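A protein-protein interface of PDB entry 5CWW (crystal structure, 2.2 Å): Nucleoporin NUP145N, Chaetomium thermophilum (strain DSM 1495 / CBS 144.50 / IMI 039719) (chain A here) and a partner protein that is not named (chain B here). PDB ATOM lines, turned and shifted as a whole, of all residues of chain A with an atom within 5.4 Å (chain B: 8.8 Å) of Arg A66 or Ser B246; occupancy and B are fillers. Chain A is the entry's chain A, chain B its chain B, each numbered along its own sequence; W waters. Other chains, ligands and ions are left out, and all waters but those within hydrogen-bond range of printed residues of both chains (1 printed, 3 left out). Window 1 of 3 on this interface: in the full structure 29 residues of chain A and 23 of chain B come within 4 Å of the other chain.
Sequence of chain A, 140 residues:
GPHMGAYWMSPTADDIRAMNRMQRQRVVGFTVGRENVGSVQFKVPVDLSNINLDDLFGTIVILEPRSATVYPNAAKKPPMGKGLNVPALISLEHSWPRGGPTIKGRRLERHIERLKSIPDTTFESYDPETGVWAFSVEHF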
ATOM      1  N   VAL A  37       4.667  -3.801  13.293  1.00  0.00           N
ATOM      2  CA  VAL A  37       5.876  -4.281  13.957  1.00  0.00           C
ATOM      3  C   VAL A  37       5.722  -5.747  14.350  1.00  0.00           C
ATOM      4  O   VAL A  37       6.495  -6.598  13.912  1.00  0.00           O
ATOM      5  CB  VAL A  37       6.208  -3.444  15.210  1.00  0.00           C
ATOM      6  CG1 VAL A  37       7.497  -3.936  15.864  1.00  0.00           C
ATOM      7  CG2 VAL A  37       6.326  -1.970  14.847  1.00  0.00           C
ATOM      8  N   GLU A  64      10.092  -3.191  18.511  1.00  0.00           N
ATOM      9  CA  GLU A  64      10.718  -2.370  17.484  1.00  0.00           C
ATOM     10  C   GLU A  64      10.812  -3.185  16.203  1.00  0.00           C
ATOM     11  O   GLU A  64      10.642  -4.403  16.233  1.00  0.00           O
ATOM     12  CB  GLU A  64      12.107  -1.899  17.926  1.00  0.00           C
ATOM     13  CG  GLU A  64      12.089  -0.778  18.955  1.00  0.00           C
ATOM     14  CD  GLU A  64      13.484  -0.311  19.337  1.00  0.00           C
ATOM     15  OE1 GLU A  64      14.469  -0.946  18.905  1.00  0.00           O
ATOM     16  OE2 GLU A  64      13.595   0.693  20.071  1.00  0.00           O
ATOM     17  N   PRO A  65      11.077  -2.519  15.066  1.00  0.00           N
ATOM     18  CA  PRO A  65      11.200  -3.267  13.810  1.00  0.00           C
ATOM     19  C   PRO A  65      12.148  -4.457  13.927  1.00  0.00           C
ATOM     20  O   PRO A  65      13.318  -4.284  14.269  1.00  0.00           O
ATOM     21  CB  PRO A  65      11.743  -2.221  12.836  1.00  0.00           C
ATOM     22  CG  PRO A  65      11.219  -0.930  13.354  1.00  0.00           C
ATOM     23  CD  PRO A  65      11.193  -1.065  14.854  1.00  0.00           C
ATOM     24  N   ARG A  66      11.617  -5.649  13.674  1.00  0.00           N
ATOM     25  CA  ARG A  66      12.387  -6.889  13.734  1.00  0.00           C
ATOM     26  C   ARG A  66      12.935  -7.184  15.128  1.00  0.00           C
ATOM     27  O   ARG A  66      13.941  -7.881  15.257  1.00  0.00           O
ATOM     28  CB  ARG A  66      13.547  -6.848  12.729  1.00  0.00           C
ATOM     29  CG  ARG A  66      13.125  -6.705  11.277  1.00  0.00           C
ATOM     30  CD  ARG A  66      14.308  -6.310  10.400  1.00  0.00           C
ATOM     31  NE  ARG A  66      15.391  -7.290  10.448  1.00  0.00           N
ATOM     32  CZ  ARG A  66      15.517  -8.328   9.623  1.00  0.00           C
ATOM     33  NH1 ARG A  66      14.623  -8.548   8.666  1.00  0.00           N
ATOM     34  NH2 ARG A  66      16.545  -9.155   9.759  1.00  0.00           N
ATOM     35  N   SER A  67      12.287  -6.667  16.171  1.00  0.00           N
ATOM     36  CA  SER A  67      12.776  -6.875  17.534  1.00  0.00           C
ATOM     37  C   SER A  67      11.665  -6.895  18.584  1.00  0.00           C
ATOM     38  O   SER A  67      10.873  -5.958  18.690  1.00  0.00           O
ATOM     39  CB  SER A  67      13.794  -5.794  17.898  1.00  0.00           C
ATOM     40  OG  SER A  67      14.402  -6.074  19.147  1.00  0.00           O
ATOM     41  N   ALA A  68      11.628  -7.977  19.356  1.00  0.00           N
ATOM     42  CA  ALA A  68      10.724  -8.098  20.493  1.00  0.00           C
ATOM     43  C   ALA A  68      11.523  -8.385  21.759  1.00  0.00           C
ATOM     44  O   ALA A  68      12.308  -9.334  21.805  1.00  0.00           O
ATOM     45  CB  ALA A  68       9.702  -9.195  20.251  1.00  0.00           C
ATOM     46  N   LEU A  92       6.857 -11.417  14.398  1.00  0.00           N
ATOM     47  CA  LEU A  92       7.618 -10.259  13.941  1.00  0.00           C
ATOM     48  C   LEU A  92       7.463 -10.048  12.441  1.00  0.00           C
ATOM     49  O   LEU A  92       7.817 -10.912  11.638  1.00  0.00           O
ATOM     50  CB  LEU A  92       9.098 -10.416  14.294  1.00  0.00           C
ATOM     51  CG  LEU A  92       9.475 -10.241  15.766  1.00  0.00           C
ATOM     52  CD1 LEU A  92      10.961 -10.499  15.953  1.00  0.00           C
ATOM     53  CD2 LEU A  92       9.109  -8.852  16.271  1.00  0.00           C
ATOM     54  N   GLU A  93       6.930  -8.890  12.075  1.00  0.00           N
ATOM     55  CA  GLU A  93       6.844  -8.498  10.678  1.00  0.00           C
ATOM     56  C   GLU A  93       8.218  -8.071  10.168  1.00  0.00           C
ATOM     57  O   GLU A  93       9.128  -7.821  10.957  1.00  0.00           O
ATOM     58  CB  GLU A  93       5.830  -7.365  10.505  1.00  0.00           C
ATOM     59  CG  GLU A  93       4.436  -7.711  11.016  1.00  0.00           C
ATOM     60  CD  GLU A  93       3.438  -6.589  10.820  1.00  0.00           C
ATOM     61  OE1 GLU A  93       3.571  -5.833   9.835  1.00  0.00           O
ATOM     62  OE2 GLU A  93       2.519  -6.462  11.657  1.00  0.00           O
ATOM     63  N   HIS A  94       8.357  -8.000   8.848  1.00  0.00           N
ATOM     64  CA  HIS A  94       9.599  -7.560   8.213  1.00  0.00           C
ATOM     65  C   HIS A  94      10.790  -8.463   8.539  1.00  0.00           C
ATOM     66  O   HIS A  94      11.932  -8.006   8.523  1.00  0.00           O
ATOM     67  CB  HIS A  94       9.928  -6.124   8.629  1.00  0.00           C
ATOM     68  CG  HIS A  94       8.748  -5.203   8.616  1.00  0.00           C
ATOM     69  ND1 HIS A  94       8.058  -4.893   7.464  1.00  0.00           N
ATOM     70  CD2 HIS A  94       8.139  -4.522   9.614  1.00  0.00           C
ATOM     71  CE1 HIS A  94       7.073  -4.062   7.755  1.00  0.00           C
ATOM     72  NE2 HIS A  94       7.100  -3.822   9.054  1.00  0.00           N
ATOM     73  N   SER A  95      10.524  -9.734   8.837  1.00  0.00           N
ATOM     74  CA  SER A  95      11.577 -10.673   9.224  1.00  0.00           C
ATOM     75  C   SER A  95      12.133 -11.464   8.036  1.00  0.00           C
ATOM     76  O   SER A  95      12.482 -12.638   8.167  1.00  0.00           O
ATOM     77  CB  SER A  95      11.048 -11.640  10.285  1.00  0.00           C
ATOM     78  OG  SER A  95      10.710 -10.947  11.476  1.00  0.00           O
ATOM     79  N   TRP A  96      12.219 -10.811   6.882  1.00  0.00           N
ATOM     80  CA  TRP A  96      12.809 -11.416   5.689  1.00  0.00           C
ATOM     81  C   TRP A  96      14.325 -11.252   5.717  1.00  0.00           C
ATOM     82  O   TRP A  96      14.853 -10.542   6.574  1.00  0.00           O
ATOM     83  CB  TRP A  96      12.225 -10.795   4.413  1.00  0.00           C
ATOM     84  CG  TRP A  96      12.055  -9.322   4.482  1.00  0.00           C
ATOM     85  CD1 TRP A  96      13.038  -8.394   4.636  1.00  0.00           C
ATOM     86  CD2 TRP A  96      10.825  -8.598   4.400  1.00  0.00           C
ATOM     87  NE1 TRP A  96      12.498  -7.133   4.656  1.00  0.00           N
ATOM     88  CE2 TRP A  96      11.139  -7.231   4.513  1.00  0.00           C
ATOM     89  CE3 TRP A  96       9.489  -8.974   4.242  1.00  0.00           C
ATOM     90  CZ2 TRP A  96      10.167  -6.238   4.471  1.00  0.00           C
ATOM     91  CZ3 TRP A  96       8.526  -7.988   4.203  1.00  0.00           C
ATOM     92  CH2 TRP A  96       8.870  -6.635   4.317  1.00  0.00           C
ATOM     93  N   PRO A  97      15.035 -11.924   4.794  1.00  0.00           N
ATOM     94  CA  PRO A  97      16.482 -11.704   4.697  1.00  0.00           C
ATOM     95  C   PRO A  97      16.803 -10.229   4.507  1.00  0.00           C
ATOM     96  O   PRO A  97      16.031  -9.517   3.865  1.00  0.00           O
ATOM     97  CB  PRO A  97      16.885 -12.515   3.462  1.00  0.00           C
ATOM     98  CG  PRO A  97      15.831 -13.541   3.311  1.00  0.00           C
ATOM     99  CD  PRO A  97      14.565 -12.935   3.829  1.00  0.00           C
ATOM    100  N   ARG A  98      17.920  -9.776   5.066  1.00  0.00           N
ATOM    101  CA  ARG A  98      18.304  -8.374   4.957  1.00  0.00           C
ATOM    102  C   ARG A  98      18.501  -7.950   3.503  1.00  0.00           C
ATOM    103  O   ARG A  98      18.480  -6.759   3.193  1.00  0.00           O
ATOM    104  CB  ARG A  98      19.579  -8.107   5.757  1.00  0.00           C
ATOM    105  CG  ARG A  98      19.331  -7.840   7.235  1.00  0.00           C
ATOM    106  CD  ARG A  98      18.743  -6.453   7.448  1.00  0.00           C
ATOM    107  NE  ARG A  98      18.431  -6.184   8.848  1.00  0.00           N
ATOM    108  CZ  ARG A  98      17.834  -5.077   9.280  1.00  0.00           C
ATOM    109  NH1 ARG A  98      17.588  -4.916  10.572  1.00  0.00           N
ATOM    110  NH2 ARG A  98      17.487  -4.126   8.424  1.00  0.00           N
ATOM    111  N   ILE A 118      17.540 -20.204  15.731  1.00  0.00           N
ATOM    112  CA  ILE A 118      17.693 -19.178  16.761  1.00  0.00           C
ATOM    113  C   ILE A 118      17.423 -19.802  18.132  1.00  0.00           C
ATOM    114  O   ILE A 118      16.349 -20.356  18.356  1.00  0.00           O
ATOM    115  CB  ILE A 118      16.750 -17.978  16.530  1.00  0.00           C
ATOM    116  CG1 ILE A 118      17.181 -17.216  15.275  1.00  0.00           C
ATOM    117  CG2 ILE A 118      16.772 -17.033  17.731  1.00  0.00           C
ATOM    118  CD1 ILE A 118      16.259 -16.079  14.878  1.00  0.00           C
ATOM    119  N   TRP A 133       7.637 -13.573  10.750  1.00  0.00           N
ATOM    120  CA  TRP A 133       8.257 -14.673  11.475  1.00  0.00           C
ATOM    121  C   TRP A 133       7.508 -14.923  12.784  1.00  0.00           C
ATOM    122  O   TRP A 133       7.418 -14.035  13.635  1.00  0.00           O
ATOM    123  CB  TRP A 133       9.729 -14.365  11.754  1.00  0.00           C
ATOM    124  CG  TRP A 133      10.399 -15.329  12.687  1.00  0.00           C
ATOM    125  CD1 TRP A 133      10.227 -16.684  12.737  1.00  0.00           C
ATOM    126  CD2 TRP A 133      11.346 -15.007  13.711  1.00  0.00           C
ATOM    127  NE1 TRP A 133      11.014 -17.224  13.727  1.00  0.00           N
ATOM    128  CE2 TRP A 133      11.711 -16.216  14.337  1.00  0.00           C
ATOM    129  CE3 TRP A 133      11.924 -13.815  14.155  1.00  0.00           C
ATOM    130  CZ2 TRP A 133      12.622 -16.263  15.390  1.00  0.00           C
ATOM    131  CZ3 TRP A 133      12.830 -13.865  15.197  1.00  0.00           C
ATOM    132  CH2 TRP A 133      13.171 -15.081  15.803  1.00  0.00           C
ATOM    133  N   LYS B 222      21.615  -2.301  14.473  1.00  0.00           N
ATOM    134  CA  LYS B 222      20.321  -2.953  14.293  1.00  0.00           C
ATOM    135  C   LYS B 222      19.182  -1.934  14.355  1.00  0.00           C
ATOM    136  O   LYS B 222      18.169  -2.088  13.674  1.00  0.00           O
ATOM    137  CB  LYS B 222      20.123  -4.046  15.342  1.00  0.00           C
ATOM    138  CG  LYS B 222      21.211  -5.114  15.320  1.00  0.00           C
ATOM    139  CD  LYS B 222      20.898  -6.268  16.262  1.00  0.00           C
ATOM    140  CE  LYS B 222      20.720  -5.798  17.704  1.00  0.00           C
ATOM    141  NZ  LYS B 222      21.907  -5.033  18.189  1.00  0.00           N
ATOM    142  N   LYS B 223      19.350  -0.900  15.175  1.00  0.00           N
ATOM    143  CA  LYS B 223      18.391   0.197  15.220  1.00  0.00           C
ATOM    144  C   LYS B 223      18.553   1.066  13.979  1.00  0.00           C
ATOM    145  O   LYS B 223      17.576   1.422  13.319  1.00  0.00           O
ATOM    146  CB  LYS B 223      18.578   1.050  16.480  1.00  0.00           C
ATOM    147  CG  LYS B 223      18.436   0.298  17.798  1.00  0.00           C
ATOM    148  CD  LYS B 223      18.421   1.269  18.975  1.00  0.00           C
ATOM    149  CE  LYS B 223      18.332   0.555  20.320  1.00  0.00           C
ATOM    150  NZ  LYS B 223      19.648   0.020  20.777  1.00  0.00           N
ATOM    151  N   ALA B 225      19.754   0.387  11.038  1.00  0.00           N
ATOM    152  CA  ALA B 225      19.408  -0.255   9.770  1.00  0.00           C
ATOM    153  C   ALA B 225      17.946  -0.025   9.402  1.00  0.00           C
ATOM    154  O   ALA B 225      17.604   0.077   8.224  1.00  0.00           O
ATOM    155  CB  ALA B 225      19.701  -1.750   9.837  1.00  0.00           C
ATOM    156  N   ASP B 226      17.092   0.070  10.414  1.00  0.00           N
ATOM    157  CA  ASP B 226      15.649   0.139  10.202  1.00  0.00           C
ATOM    158  C   ASP B 226      15.097   1.541  10.445  1.00  0.00           C
ATOM    159  O   ASP B 226      13.890   1.761  10.374  1.00  0.00           O
ATOM    160  CB  ASP B 226      14.944  -0.868  11.110  1.00  0.00           C
ATOM    161  CG  ASP B 226      15.436  -2.286  10.891  1.00  0.00           C
ATOM    162  OD1 ASP B 226      15.584  -2.689   9.718  1.00  0.00           O
ATOM    163  OD2 ASP B 226      15.684  -2.992  11.891  1.00  0.00           O
ATOM    164  N   LYS B 243      18.639  -9.816  26.601  1.00  0.00           N
ATOM    165  CA  LYS B 243      18.508  -9.887  25.151  1.00  0.00           C
ATOM    166  C   LYS B 243      17.082 -10.236  24.740  1.00  0.00           C
ATOM    167  O   LYS B 243      16.424 -11.061  25.375  1.00  0.00           O
ATOM    168  CB  LYS B 243      19.482 -10.918  24.579  1.00  0.00           C
ATOM    169  CG  LYS B 243      20.945 -10.613  24.868  1.00  0.00           C
ATOM    170  CD  LYS B 243      21.540 -11.606  25.859  1.00  0.00           C
ATOM    171  CE  LYS B 243      23.007 -11.308  26.139  1.00  0.00           C
ATOM    172  NZ  LYS B 243      23.195  -9.980  26.788  1.00  0.00           N
ATOM    173  N   GLY B 244      16.613  -9.594  23.676  1.00  0.00           N
ATOM    174  CA  GLY B 244      15.315  -9.896  23.100  1.00  0.00           C
ATOM    175  C   GLY B 244      15.432 -10.908  21.975  1.00  0.00           C
ATOM    176  O   GLY B 244      16.359 -11.721  21.951  1.00  0.00           O
ATOM    177  N   PHE B 245      14.496 -10.845  21.033  1.00  0.00           N
ATOM    178  CA  PHE B 245      14.449 -11.792  19.925  1.00  0.00           C
ATOM    179  C   PHE B 245      14.345 -11.062  18.595  1.00  0.00           C
ATOM    180  O   PHE B 245      13.527 -10.157  18.432  1.00  0.00           O
ATOM    181  CB  PHE B 245      13.275 -12.751  20.098  1.00  0.00           C
ATOM    182  CG  PHE B 245      13.395 -13.629  21.308  1.00  0.00           C
ATOM    183  CD1 PHE B 245      14.112 -14.813  21.250  1.00  0.00           C
ATOM    184  CD2 PHE B 245      12.797 -13.272  22.503  1.00  0.00           C
ATOM    185  CE1 PHE B 245      14.228 -15.624  22.361  1.00  0.00           C
ATOM    186  CE2 PHE B 245      12.909 -14.079  23.618  1.00  0.00           C
ATOM    187  CZ  PHE B 245      13.627 -15.258  23.545  1.00  0.00           C
ATOM    188  N   SER B 246      15.180 -11.468  17.647  1.00  0.00           N
ATOM    189  CA  SER B 246      15.272 -10.790  16.363  1.00  0.00           C
ATOM    190  C   SER B 246      15.957 -11.669  15.314  1.00  0.00           C
ATOM    191  O   SER B 246      16.890 -12.402  15.639  1.00  0.00           O
ATOM    192  CB  SER B 246      16.040  -9.478  16.523  1.00  0.00           C
ATOM    193  OG  SER B 246      16.419  -8.945  15.265  1.00  0.00           O
ATOM    194  N   PRO B 247      15.497 -11.603  14.051  1.00  0.00           N
ATOM    195  CA  PRO B 247      16.203 -12.326  12.986  1.00  0.00           C
ATOM    196  C   PRO B 247      17.621 -11.804  12.802  1.00  0.00           C
ATOM    197  O   PRO B 247      18.489 -12.513  12.292  1.00  0.00           O
ATOM    198  CB  PRO B 247      15.354 -12.048  11.742  1.00  0.00           C
ATOM    199  CG  PRO B 247      14.602 -10.803  12.059  1.00  0.00           C
ATOM    200  CD  PRO B 247      14.333 -10.866  13.530  1.00  0.00           C
ATOM    201  N   ASP B 248      17.847 -10.564  13.224  1.00  0.00           N
ATOM    202  CA  ASP B 248      19.162  -9.950  13.118  1.00  0.00           C
ATOM    203  C   ASP B 248      20.158 -10.567  14.099  1.00  0.00           C
ATOM    204  O   ASP B 248      21.338 -10.225  14.087  1.00  0.00           O
ATOM    205  CB  ASP B 248      19.052  -8.444  13.353  1.00  0.00           C
ATOM    206  CG  ASP B 248      18.371  -7.727  12.203  1.00  0.00           C
ATOM    207  OD1 ASP B 248      18.750  -7.975  11.038  1.00  0.00           O
ATOM    208  OD2 ASP B 248      17.446  -6.929  12.459  1.00  0.00           O
ATOM    209  N   ALA B 249      19.683 -11.486  14.935  1.00  0.00           N
ATOM    210  CA  ALA B 249      20.568 -12.257  15.799  1.00  0.00           C
ATOM    211  C   ALA B 249      21.581 -13.045  14.966  1.00  0.00           C
ATOM    212  O   ALA B 249      22.709 -13.273  15.405  1.00  0.00           O
ATOM    213  CB  ALA B 249      19.763 -13.195  16.686  1.00  0.00           C
ATOM    214  N   PHE B 250      21.172 -13.457  13.767  1.00  0.00           N
ATOM    215  CA  PHE B 250      22.074 -14.149  12.846  1.00  0.00           C
ATOM    216  C   PHE B 250      22.368 -13.317  11.601  1.00  0.00           C
ATOM    217  O   PHE B 250      23.466 -13.383  11.055  1.00  0.00           O
ATOM    218  CB  PHE B 250      21.494 -15.508  12.434  1.00  0.00           C
ATOM    219  CG  PHE B 250      20.211 -15.421  11.652  1.00  0.00           C
ATOM    220  CD1 PHE B 250      20.225 -15.148  10.295  1.00  0.00           C
ATOM    221  CD2 PHE B 250      18.990 -15.640  12.272  1.00  0.00           C
ATOM    222  CE1 PHE B 250      19.048 -15.072   9.574  1.00  0.00           C
ATOM    223  CE2 PHE B 250      17.810 -15.568  11.556  1.00  0.00           C
ATOM    224  CZ  PHE B 250      17.840 -15.284  10.206  1.00  0.00           C
ATOM    225  N   ASP B 251      21.397 -12.527  11.157  1.00  0.00           N
ATOM    226  CA  ASP B 251      21.539 -11.804   9.898  1.00  0.00           C
ATOM    227  C   ASP B 251      22.438 -10.581  10.047  1.00  0.00           C
ATOM    228  O   ASP B 251      23.008 -10.105   9.063  1.00  0.00           O
ATOM    229  CB  ASP B 251      20.169 -11.380   9.360  1.00  0.00           C
ATOM    230  CG  ASP B 251      20.043 -11.568   7.851  1.00  0.00           C
ATOM    231  OD1 ASP B 251      21.046 -11.908   7.188  1.00  0.00           O
ATOM    232  OD2 ASP B 251      18.930 -11.363   7.322  1.00  0.00           O
ATOM    233  N   MET B 252      22.567 -10.080  11.274  1.00  0.00           N
ATOM    234  CA  MET B 252      23.497  -8.992  11.557  1.00  0.00           C
ATOM    235  C   MET B 252      24.490  -9.398  12.643  1.00  0.00           C
ATOM    236  O   MET B 252      24.956  -8.563  13.418  1.00  0.00           O
ATOM    237  CB  MET B 252      22.741  -7.725  11.966  1.00  0.00           C
ATOM    238  CG  MET B 252      21.942  -7.102  10.825  1.00  0.00           C
ATOM    239  SD  MET B 252      21.290  -5.459  11.193  1.00  0.00           S
ATOM    240  CE  MET B 252      22.794  -4.483  11.124  1.00  0.00           C
ATOM    241  N   GLU B 253      24.799 -10.690  12.702  1.00  0.00           N
ATOM    242  CA  GLU B 253      25.894 -11.165  13.537  1.00  0.00           C
ATOM    243  C   GLU B 253      27.204 -10.783  12.857  1.00  0.00           C
ATOM    244  O   GLU B 253      27.498 -11.259  11.764  1.00  0.00           O
ATOM    245  CB  GLU B 253      25.815 -12.677  13.750  1.00  0.00           C
ATOM    246  CG  GLU B 253      26.877 -13.224  14.693  1.00  0.00           C
ATOM    247  CD  GLU B 253      26.882 -14.737  14.756  1.00  0.00           C
ATOM    248  OE1 GLU B 253      26.624 -15.288  15.845  1.00  0.00           O
ATOM    249  OE2 GLU B 253      27.150 -15.377  13.718  1.00  0.00           O
ATOM    250  N   SER B 278      26.426 -13.857   8.105  1.00  0.00           N
ATOM    251  CA  SER B 278      25.349 -14.212   7.190  1.00  0.00           C
ATOM    252  C   SER B 278      25.787 -14.068   5.734  1.00  0.00           C
ATOM    253  O   SER B 278      25.147 -14.610   4.836  1.00  0.00           O
ATOM    254  CB  SER B 278      24.120 -13.340   7.448  1.00  0.00           C
ATOM    255  OG  SER B 278      24.394 -11.984   7.139  1.00  0.00           O
ATOM    256  N   ASP B 280      26.582 -10.848   4.446  1.00  0.00           N
ATOM    257  CA  ASP B 280      26.330  -9.471   4.039  1.00  0.00           C
ATOM    258  C   ASP B 280      27.474  -8.542   4.421  1.00  0.00           C
ATOM    259  O   ASP B 280      28.220  -8.801   5.369  1.00  0.00           O
ATOM    260  CB  ASP B 280      25.023  -8.964   4.652  1.00  0.00           C
ATOM    261  CG  ASP B 280      23.807  -9.705   4.130  1.00  0.00           C
ATOM    262  OD1 ASP B 280      23.872 -10.244   3.006  1.00  0.00           O
ATOM    263  OD2 ASP B 280      22.781  -9.744   4.842  1.00  0.00           O
ATOM    264  N   TYR B 282      28.479  -4.304   4.988  1.00  0.00           N
ATOM    265  CA  TYR B 282      27.944  -2.979   5.268  1.00  0.00           C
ATOM    266  C   TYR B 282      29.064  -1.950   5.348  1.00  0.00           C
ATOM    267  O   TYR B 282      30.221  -2.297   5.581  1.00  0.00           O
ATOM    268  CB  TYR B 282      27.163  -2.980   6.584  1.00  0.00           C
ATOM    269  CG  TYR B 282      25.880  -3.775   6.556  1.00  0.00           C
ATOM    270  CD1 TYR B 282      25.875  -5.131   6.850  1.00  0.00           C
ATOM    271  CD2 TYR B 282      24.671  -3.165   6.256  1.00  0.00           C
ATOM    272  CE1 TYR B 282      24.702  -5.859   6.836  1.00  0.00           C
ATOM    273  CE2 TYR B 282      23.494  -3.885   6.238  1.00  0.00           C
ATOM    274  CZ  TYR B 282      23.514  -5.230   6.530  1.00  0.00           C
ATOM    275  OH  TYR B 282      22.343  -5.950   6.516  1.00  0.00           O
ATOM    276  N   PRO B 372      22.590  -4.115   2.925  1.00  0.00           N
ATOM    277  CA  PRO B 372      23.640  -5.016   2.433  1.00  0.00           C
ATOM    278  C   PRO B 372      24.016  -4.727   0.984  1.00  0.00           C
ATOM    279  O   PRO B 372      23.132  -4.568   0.146  1.00  0.00           O
ATOM    280  CB  PRO B 372      23.007  -6.410   2.546  1.00  0.00           C
ATOM    281  CG  PRO B 372      21.751  -6.243   3.323  1.00  0.00           C
ATOM    282  CD  PRO B 372      21.325  -4.824   3.176  1.00  0.00           C
HETATM  283  O   HOH W   1      20.774 -11.656   4.524  1.00  0.00           O
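Hydrophobic or aromatic side chains of chain B within 4 Å of the printed part of chain A: Ala B225, Phe B245, Pro B247, Phe B250, Met B252, Tyr B282 and Pro B372. Among the printed residues, Asp or Glu carboxylates within 4 Å of a Lys or Arg side-chain nitrogen of the other chain: Arg A66 with Asp B248, Arg A98 with Asp B226 and Arg A98 with Asp B248.
The side-chain hydroxyl of Ser B246 is in hydrogen-bond range of the backbone carbonyl oxygen of Arg A66, at 2.7 Å. NH2 of Arg A66 is in salt-bridge range of OD1 of Asp B248 (2.8 Å). The backbone carbonyl oxygen of Ala A68 is in hydrogen-bond range of the backbone NH of Phe B245 (2.8 Å). The side-chain carboxylate of Asp B226 lies within salt-bridge range of the guanidinium group of Arg A98 (2.7 Å). OD2 of Asp B248 is in salt-bridge range of NH1 of Arg A98 (2.8 Å). N of Arg A98 is in hydrogen-bond range of OD2 of Asp B251 (2.9 Å). The guanidinium group of Arg A98 sits at hydrogen-bond distance from the side-chain sulfur of Met B252 (3.8 Å).
Water W1 lies within hydrogen-bond range of the side-chain carboxylate (OD1) of Asp B251, the side-chain carboxylate (OD2) of Asp B280 and the backbone NH (N) of Arg A98.
Of chain B, only Asp B226 (3.9 Å), Phe B245 (3.9 Å), Ser B246 (2.7 Å), Pro B247 (3.4 Å) and Asp B248 (2.8 Å) come within 4 Å of Arg A66. Ser A67 touches just one residue of chain B: Phe B245. Printed residues of chain B within 4 Å of Ala A68: Gly B244 and Phe B245. Of the printed residues of chain B, Ser A95 touches Pro B247 (3.9 Å). Of the printed residues of chain A, Gly B244 touches Ala A68. Ser B246 touches three residues of chain A. Printed residues of chain A within 4 Å of Asp B280: Arg A98 (3.7 Å). The nearest residue of chain B that does not touch Arg A66 is Asp B251 (4.1 Å). The nearest printed residue of chain A that does not touch Asp B226 is Glu A64 (6.5 Å).
The backbone carbonyl oxygen of His A94 sits at hydrogen-bond distance from the guanidinium group of Arg A66 (2.7 Å). NH1 of Arg A66 is in hydrogen-bond range of O of Trp A96, 2.9 Å away. The backbone carbonyl oxygen (O) of Leu A92 sits at hydrogen-bond distance from the side-chain hydroxyl (OG) of Ser A95 (2.9 Å). O of Trp A133 lies within hydrogen-bond range of N of Leu A92 (2.8 Å). The backbone NH (N) of Asp B248 is in hydrogen-bond range of the side-chain hydroxyl (OG) of Ser B246, at 3.0 Å. O of Asp B251 sits at hydrogen-bond distance from OG of Ser B278 (3.0 Å).
Among the printed residues, merely in contact across the chains: Arg A98 with Pro B372, Ala A68 with Gly B244, Arg A66 with Pro B247, Ser A67 with Phe B245, Arg A98 with Ala B225, Leu A92 with Phe B245, Arg A98 with Tyr B282, Pro A65 with Asp B226, Pro A97 with Asp B251, Trp A133 with Pro B247, Ile A118 with Phe B250, Arg A98 with Asp B280, Ile A118 with Ser B246, Trp A133 with Ser B246, Arg A66 with Asp B226, Arg A66 with Phe B245 and Ser A95 with Pro B247.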
